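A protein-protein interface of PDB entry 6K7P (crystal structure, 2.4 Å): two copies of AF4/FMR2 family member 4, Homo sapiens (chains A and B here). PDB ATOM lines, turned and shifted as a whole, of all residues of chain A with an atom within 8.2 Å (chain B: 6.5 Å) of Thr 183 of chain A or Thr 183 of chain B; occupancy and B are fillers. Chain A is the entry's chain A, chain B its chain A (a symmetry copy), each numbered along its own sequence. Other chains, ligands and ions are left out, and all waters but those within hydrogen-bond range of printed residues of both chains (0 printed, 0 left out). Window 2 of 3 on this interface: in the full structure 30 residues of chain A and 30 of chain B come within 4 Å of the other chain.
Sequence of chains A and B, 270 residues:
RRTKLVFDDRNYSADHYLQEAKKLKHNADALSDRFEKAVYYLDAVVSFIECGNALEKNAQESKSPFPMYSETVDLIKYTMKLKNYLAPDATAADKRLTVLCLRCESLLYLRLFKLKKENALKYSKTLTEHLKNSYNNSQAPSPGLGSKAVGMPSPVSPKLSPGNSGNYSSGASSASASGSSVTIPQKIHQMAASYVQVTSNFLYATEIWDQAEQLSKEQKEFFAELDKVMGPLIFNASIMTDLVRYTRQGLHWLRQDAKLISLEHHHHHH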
ATOM      1  N   HIS A 130     -27.758  -4.403  22.068  1.00  0.00           N
ATOM      2  CA  HIS A 130     -27.380  -5.549  22.890  1.00  0.00           C
ATOM      3  C   HIS A 130     -26.659  -6.617  22.081  1.00  0.00           C
ATOM      4  O   HIS A 130     -25.831  -7.353  22.632  1.00  0.00           O
ATOM      5  CB  HIS A 130     -28.612  -6.141  23.569  1.00  0.00           C
ATOM      6  CG  HIS A 130     -29.073  -5.361  24.755  1.00  0.00           C
ATOM      7  ND1 HIS A 130     -29.340  -4.009  24.698  1.00  0.00           N
ATOM      8  CD2 HIS A 130     -29.297  -5.736  26.036  1.00  0.00           C
ATOM      9  CE1 HIS A 130     -29.719  -3.589  25.891  1.00  0.00           C
ATOM     10  NE2 HIS A 130     -29.703  -4.617  26.721  1.00  0.00           N
ATOM     11  N   ASN A 133     -23.387  -5.448  22.762  1.00  0.00           N
ATOM     12  CA  ASN A 133     -22.969  -5.653  24.152  1.00  0.00           C
ATOM     13  C   ASN A 133     -22.645  -7.119  24.423  1.00  0.00           C
ATOM     14  O   ASN A 133     -21.578  -7.445  24.961  1.00  0.00           O
ATOM     15  CB  ASN A 133     -24.065  -5.183  25.115  1.00  0.00           C
ATOM     16  CG  ASN A 133     -24.272  -3.684  25.093  1.00  0.00           C
ATOM     17  OD1 ASN A 133     -23.486  -2.946  24.496  1.00  0.00           O
ATOM     18  ND2 ASN A 133     -25.340  -3.221  25.746  1.00  0.00           N
ATOM     19  N   SER A 134     -23.573  -8.020  24.080  1.00  0.00           N
ATOM     20  CA  SER A 134     -23.384  -9.440  24.369  1.00  0.00           C
ATOM     21  C   SER A 134     -22.174 -10.007  23.638  1.00  0.00           C
ATOM     22  O   SER A 134     -21.536 -10.947  24.126  1.00  0.00           O
ATOM     23  CB  SER A 134     -24.647 -10.221  23.994  1.00  0.00           C
ATOM     24  OG  SER A 134     -25.660 -10.063  24.971  1.00  0.00           O
ATOM     25  N   TYR A 135     -21.845  -9.444  22.475  1.00  0.00           N
ATOM     26  CA  TYR A 135     -20.716  -9.908  21.676  1.00  0.00           C
ATOM     27  C   TYR A 135     -19.400  -9.326  22.183  1.00  0.00           C
ATOM     28  O   TYR A 135     -18.404 -10.048  22.299  1.00  0.00           O
ATOM     29  CB  TYR A 135     -20.955  -9.544  20.207  1.00  0.00           C
ATOM     30  CG  TYR A 135     -19.869  -9.974  19.255  1.00  0.00           C
ATOM     31  CD1 TYR A 135     -19.318 -11.249  19.328  1.00  0.00           C
ATOM     32  CD2 TYR A 135     -19.405  -9.113  18.268  1.00  0.00           C
ATOM     33  CE1 TYR A 135     -18.320 -11.650  18.452  1.00  0.00           C
ATOM     34  CE2 TYR A 135     -18.415  -9.503  17.383  1.00  0.00           C
ATOM     35  CZ  TYR A 135     -17.875 -10.774  17.481  1.00  0.00           C
ATOM     36  OH  TYR A 135     -16.884 -11.175  16.610  1.00  0.00           O
ATOM     37  N   ASN A 137     -18.822  -8.678  25.117  1.00  0.00           N
ATOM     38  CA  ASN A 137     -18.599  -9.202  26.458  1.00  0.00           C
ATOM     39  C   ASN A 137     -18.281 -10.691  26.486  1.00  0.00           C
ATOM     40  O   ASN A 137     -17.914 -11.210  27.544  1.00  0.00           O
ATOM     41  CB  ASN A 137     -19.819  -8.927  27.341  1.00  0.00           C
ATOM     42  CG  ASN A 137     -19.941  -7.466  27.715  1.00  0.00           C
ATOM     43  OD1 ASN A 137     -19.300  -6.603  27.105  1.00  0.00           O
ATOM     44  ND2 ASN A 137     -20.760  -7.176  28.722  1.00  0.00           N
ATOM     45  N   SER A 138     -18.424 -11.386  25.362  1.00  0.00           N
ATOM     46  CA  SER A 138     -18.035 -12.783  25.249  1.00  0.00           C
ATOM     47  C   SER A 138     -16.616 -12.955  24.718  1.00  0.00           C
ATOM     48  O   SER A 138     -16.092 -14.075  24.738  1.00  0.00           O
ATOM     49  CB  SER A 138     -19.023 -13.525  24.339  1.00  0.00           C
ATOM     50  OG  SER A 138     -19.201 -12.833  23.112  1.00  0.00           O
ATOM     51  N   SER A 181     -19.965 -19.671  21.187  1.00  0.00           N
ATOM     52  CA  SER A 181     -21.318 -19.484  21.689  1.00  0.00           C
ATOM     53  C   SER A 181     -21.439 -18.216  22.537  1.00  0.00           C
ATOM     54  O   SER A 181     -20.467 -17.782  23.157  1.00  0.00           O
ATOM     55  CB  SER A 181     -21.757 -20.701  22.503  1.00  0.00           C
ATOM     56  OG  SER A 181     -22.997 -20.448  23.141  1.00  0.00           O
ATOM     57  N   VAL A 182     -22.638 -17.620  22.553  1.00  0.00           N
ATOM     58  CA  VAL A 182     -22.896 -16.385  23.283  1.00  0.00           C
ATOM     59  C   VAL A 182     -24.086 -16.596  24.213  1.00  0.00           C
ATOM     60  O   VAL A 182     -24.915 -17.485  24.014  1.00  0.00           O
ATOM     61  CB  VAL A 182     -23.154 -15.184  22.342  1.00  0.00           C
ATOM     62  CG1 VAL A 182     -22.902 -13.864  23.069  1.00  0.00           C
ATOM     63  CG2 VAL A 182     -22.299 -15.281  21.082  1.00  0.00           C
ATOM     64  N   THR A 183     -24.158 -15.757  25.242  1.00  0.00           N
ATOM     65  CA  THR A 183     -25.204 -15.833  26.249  1.00  0.00           C
ATOM     66  C   THR A 183     -25.901 -14.482  26.305  1.00  0.00           C
ATOM     67  O   THR A 183     -25.239 -13.440  26.360  1.00  0.00           O
ATOM     68  CB  THR A 183     -24.622 -16.228  27.622  1.00  0.00           C
ATOM     69  OG1 THR A 183     -24.300 -17.627  27.623  1.00  0.00           O
ATOM     70  CG2 THR A 183     -25.602 -15.946  28.747  1.00  0.00           C
ATOM     71  N   ILE A 184     -27.231 -14.495  26.254  1.00  0.00           N
ATOM     72  CA  ILE A 184     -28.013 -13.266  26.149  1.00  0.00           C
ATOM     73  C   ILE A 184     -29.105 -13.255  27.215  1.00  0.00           C
ATOM     74  O   ILE A 184     -29.573 -14.326  27.636  1.00  0.00           O
ATOM     75  CB  ILE A 184     -28.627 -13.116  24.748  1.00  0.00           C
ATOM     76  CG1 ILE A 184     -29.706 -14.181  24.537  1.00  0.00           C
ATOM     77  CG2 ILE A 184     -27.550 -13.221  23.683  1.00  0.00           C
ATOM     78  CD1 ILE A 184     -30.386 -14.132  23.202  1.00  0.00           C
ATOM     79  N   PRO A 185     -29.522 -12.084  27.696  1.00  0.00           N
ATOM     80  CA  PRO A 185     -30.695 -12.041  28.575  1.00  0.00           C
ATOM     81  C   PRO A 185     -31.906 -12.588  27.840  1.00  0.00           C
ATOM     82  O   PRO A 185     -32.069 -12.382  26.637  1.00  0.00           O
ATOM     83  CB  PRO A 185     -30.851 -10.550  28.901  1.00  0.00           C
ATOM     84  CG  PRO A 185     -29.506  -9.972  28.686  1.00  0.00           C
ATOM     85  CD  PRO A 185     -28.856 -10.776  27.591  1.00  0.00           C
ATOM     86  N   GLN A 186     -32.753 -13.310  28.567  1.00  0.00           N
ATOM     87  CA  GLN A 186     -33.876 -13.947  27.900  1.00  0.00           C
ATOM     88  C   GLN A 186     -34.917 -12.932  27.423  1.00  0.00           C
ATOM     89  O   GLN A 186     -35.694 -13.244  26.520  1.00  0.00           O
ATOM     90  CB  GLN A 186     -34.480 -14.993  28.832  1.00  0.00           C
ATOM     91  CG  GLN A 186     -35.466 -14.450  29.812  1.00  0.00           C
ATOM     92  CD  GLN A 186     -36.883 -14.659  29.346  1.00  0.00           C
ATOM     93  OE1 GLN A 186     -37.282 -15.784  29.038  1.00  0.00           O
ATOM     94  NE2 GLN A 186     -37.653 -13.577  29.270  1.00  0.00           N
ATOM     95  N   ILE A 188     -33.985 -10.066  25.908  1.00  0.00           N
ATOM     96  CA  ILE A 188     -33.345  -9.889  24.611  1.00  0.00           C
ATOM     97  C   ILE A 188     -33.699 -11.044  23.680  1.00  0.00           C
ATOM     98  O   ILE A 188     -33.980 -10.838  22.496  1.00  0.00           O
ATOM     99  CB  ILE A 188     -31.821  -9.746  24.805  1.00  0.00           C
ATOM    100  CG1 ILE A 188     -31.486  -8.454  25.558  1.00  0.00           C
ATOM    101  CG2 ILE A 188     -31.063  -9.862  23.496  1.00  0.00           C
ATOM    102  CD1 ILE A 188     -32.470  -7.317  25.358  1.00  0.00           C
ATOM    103  N   HIS A 189     -33.727 -12.274  24.206  1.00  0.00           N
ATOM    104  CA  HIS A 189     -34.055 -13.428  23.372  1.00  0.00           C
ATOM    105  C   HIS A 189     -35.490 -13.363  22.857  1.00  0.00           C
ATOM    106  O   HIS A 189     -35.750 -13.630  21.678  1.00  0.00           O
ATOM    107  CB  HIS A 189     -33.834 -14.716  24.151  1.00  0.00           C
ATOM    108  CG  HIS A 189     -34.006 -15.960  23.334  1.00  0.00           C
ATOM    109  ND1 HIS A 189     -35.230 -16.570  23.156  1.00  0.00           N
ATOM    110  CD2 HIS A 189     -33.103 -16.728  22.677  1.00  0.00           C
ATOM    111  CE1 HIS A 189     -35.077 -17.650  22.408  1.00  0.00           C
ATOM    112  NE2 HIS A 189     -33.796 -17.771  22.106  1.00  0.00           N
ATOM    113  N   SER B 134     -33.324 -22.962  20.878  1.00  0.00           N
ATOM    114  CA  SER B 134     -32.557 -22.472  22.021  1.00  0.00           C
ATOM    115  C   SER B 134     -33.449 -22.215  23.228  1.00  0.00           C
ATOM    116  O   SER B 134     -32.998 -22.335  24.374  1.00  0.00           O
ATOM    117  CB  SER B 134     -31.802 -21.197  21.636  1.00  0.00           C
ATOM    118  OG  SER B 134     -30.646 -21.493  20.872  1.00  0.00           O
ATOM    119  N   SER B 138     -33.541 -24.399  26.991  1.00  0.00           N
ATOM    120  CA  SER B 138     -33.176 -23.736  28.234  1.00  0.00           C
ATOM    121  C   SER B 138     -34.219 -23.930  29.329  1.00  0.00           C
ATOM    122  O   SER B 138     -33.959 -23.574  30.484  1.00  0.00           O
ATOM    123  CB  SER B 138     -32.965 -22.237  27.979  1.00  0.00           C
ATOM    124  OG  SER B 138     -34.070 -21.680  27.282  1.00  0.00           O
ATOM    125  N   SER B 181     -31.872 -16.239  31.358  1.00  0.00           N
ATOM    126  CA  SER B 181     -30.891 -16.062  30.296  1.00  0.00           C
ATOM    127  C   SER B 181     -30.811 -17.291  29.388  1.00  0.00           C
ATOM    128  O   SER B 181     -31.078 -18.411  29.825  1.00  0.00           O
ATOM    129  CB  SER B 181     -29.516 -15.758  30.888  1.00  0.00           C
ATOM    130  OG  SER B 181     -28.528 -15.765  29.872  1.00  0.00           O
ATOM    131  N   VAL B 182     -30.448 -17.073  28.117  1.00  0.00           N
ATOM    132  CA  VAL B 182     -30.365 -18.137  27.126  1.00  0.00           C
ATOM    133  C   VAL B 182     -28.980 -18.117  26.489  1.00  0.00           C
ATOM    134  O   VAL B 182     -28.275 -17.106  26.501  1.00  0.00           O
ATOM    135  CB  VAL B 182     -31.460 -18.020  26.039  1.00  0.00           C
ATOM    136  CG1 VAL B 182     -31.685 -19.367  25.352  1.00  0.00           C
ATOM    137  CG2 VAL B 182     -32.762 -17.487  26.628  1.00  0.00           C
ATOM    138  N   THR B 183     -28.596 -19.259  25.927  1.00  0.00           N
ATOM    139  CA  THR B 183     -27.293 -19.433  25.304  1.00  0.00           C
ATOM    140  C   THR B 183     -27.516 -19.888  23.870  1.00  0.00           C
ATOM    141  O   THR B 183     -28.306 -20.805  23.623  1.00  0.00           O
ATOM    142  CB  THR B 183     -26.434 -20.442  26.093  1.00  0.00           C
ATOM    143  OG1 THR B 183     -25.952 -19.826  27.297  1.00  0.00           O
ATOM    144  CG2 THR B 183     -25.248 -20.924  25.277  1.00  0.00           C
ATOM    145  N   ILE B 184     -26.851 -19.228  22.926  1.00  0.00           N
ATOM    146  CA  ILE B 184     -27.086 -19.466  21.503  1.00  0.00           C
ATOM    147  C   ILE B 184     -25.758 -19.707  20.792  1.00  0.00           C
ATOM    148  O   ILE B 184     -24.715 -19.196  21.233  1.00  0.00           O
ATOM    149  CB  ILE B 184     -27.836 -18.288  20.861  1.00  0.00           C
ATOM    150  CG1 ILE B 184     -26.928 -17.057  20.816  1.00  0.00           C
ATOM    151  CG2 ILE B 184     -29.112 -17.990  21.627  1.00  0.00           C
ATOM    152  CD1 ILE B 184     -27.548 -15.839  20.201  1.00  0.00           C
ATOM    153  N   PRO B 185     -25.740 -20.490  19.713  1.00  0.00           N
ATOM    154  CA  PRO B 185     -24.517 -20.581  18.907  1.00  0.00           C
ATOM    155  C   PRO B 185     -24.155 -19.208  18.371  1.00  0.00           C
ATOM    156  O   PRO B 185     -25.025 -18.407  18.025  1.00  0.00           O
ATOM    157  CB  PRO B 185     -24.895 -21.552  17.782  1.00  0.00           C
ATOM    158  CG  PRO B 185     -26.021 -22.344  18.325  1.00  0.00           C
ATOM    159  CD  PRO B 185     -26.771 -21.442  19.271  1.00  0.00           C
ATOM    160  N   HIS B 189     -25.945 -16.005  16.592  1.00  0.00           N
ATOM    161  CA  HIS B 189     -25.833 -14.640  17.101  1.00  0.00           C
ATOM    162  C   HIS B 189     -25.480 -13.651  15.994  1.00  0.00           C
ATOM    163  O   HIS B 189     -26.063 -12.563  15.910  1.00  0.00           O
ATOM    164  CB  HIS B 189     -24.794 -14.579  18.211  1.00  0.00           C
ATOM    165  CG  HIS B 189     -24.710 -13.249  18.895  1.00  0.00           C
ATOM    166  ND1 HIS B 189     -23.914 -12.222  18.432  1.00  0.00           N
ATOM    167  CD2 HIS B 189     -25.296 -12.789  20.028  1.00  0.00           C
ATOM    168  CE1 HIS B 189     -24.027 -11.181  19.240  1.00  0.00           C
ATOM    169  NE2 HIS B 189     -24.857 -11.500  20.218  1.00  0.00           N
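OG of Ser 181 of chain A is in hydrogen-bond range of O of Ile 184 of chain B (2.9 Å). The backbone carbonyl oxygen (O) of Val 182 of chain A lies within hydrogen-bond range of the backbone NH (N) of Ile 184 of chain B (2.8 Å). The side-chain hydroxyl (OG1) of Thr 183 of chain A is in hydrogen-bond range of the side-chain hydroxyl (OG1) of Thr 183 of chain B (2.8 Å). O of Ile 184 of chain A lies within hydrogen-bond range of OG of Ser 181 of chain B. The backbone NH (N) of Ile 184 of chain A sits at hydrogen-bond distance from the backbone carbonyl oxygen (O) of Val 182 of chain B (2.8 Å).
O of Ser 134 of chain A sits at hydrogen-bond distance from OG of Ser 138 of chain A (3.2 Å). The side-chain hydroxyl (OG) of Ser 138 of chain A is in hydrogen-bond range of the backbone carbonyl oxygen (O) of Tyr 135 of chain A (3.0 Å). The side-chain hydroxyl (OG) of Ser 138 of chain B is in hydrogen-bond range of the backbone carbonyl oxygen (O) of Ser 134 of chain B, 3.2 Å away.
Ser 134 of chain A touches His 189 of chain B (CB to NE2, 3.99 Å). Tyr 135 of chain A touches His 189 of chain B. Thr 183 of chain B touches Ser 181 of chain A (CG2 to OG, 3.1 Å). CA of Thr 183 of chain B touches O of Val 182 of chain A, at 3.3 Å. CG2 of Val 182 of chain A touches CG of His 189 of chain B, at 3.8 Å. CG2 of Thr 183 of chain A touches OG of Ser 181 of chain B (3.1 Å). N of Gln 186 of chain A touches CA of Ser 181 of chain B, 3.7 Å away. Gln 186 of chain A touches Val 182 of chain B. His 189 of chain A touches Ser 134 of chain B (NE2 to CB, 3.99 Å). CG of His 189 of chain A touches CG2 of Val 182 of chain B, 3.8 Å away.
Of the printed residues of chain A, Ile 184 of chain B touches Ser 181 and Val 182. Of the printed residues of chain B, Ile 184 of chain A touches Ser 181 and Val 182. Printed residues of chain B within 4 Å of Val 182 of chain A: Thr 183 (3.3 Å), Ile 184 (2.8 Å) and His 189 (3.8 Å). Asn 133 of chain A touches none of the printed residues of chain B. Pro 185 of chain B touches none of the printed residues of chain A. The nearest printed residue of chain A that does not touch His 189 of chain B is Ile 184 of chain A (4.3 Å).
Of the 14 printed residues of chain A, 8 touch a printed residue of chain B. Hydrophobic or aromatic side chains of chain A that line the printed part of chain B: Tyr 135, Val 182, Ile 184 and His 189. Of the 8 printed residues of chain B, 6 touch a printed residue of chain A.
Ser 134 of chain A touches His 189 of chain B, and with the chains exchanged His 189 of chain A touches Ser 134 of chain B. Ser 181 of chain A touches Ile 184 of chain B, and with the chains exchanged Ile 184 of chain A touches Ser 181 of chain B. Val 182 of chain A touches Ile 184 of chain B, and with the chains exchanged Ile 184 of chain A touches Val 182 of chain B. Thr 183 of chain A touches its own counterpart, Thr 183 of chain B. Positions printed for both chains: 134, 138, 181, 182, 183, 184, 185 and 189.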
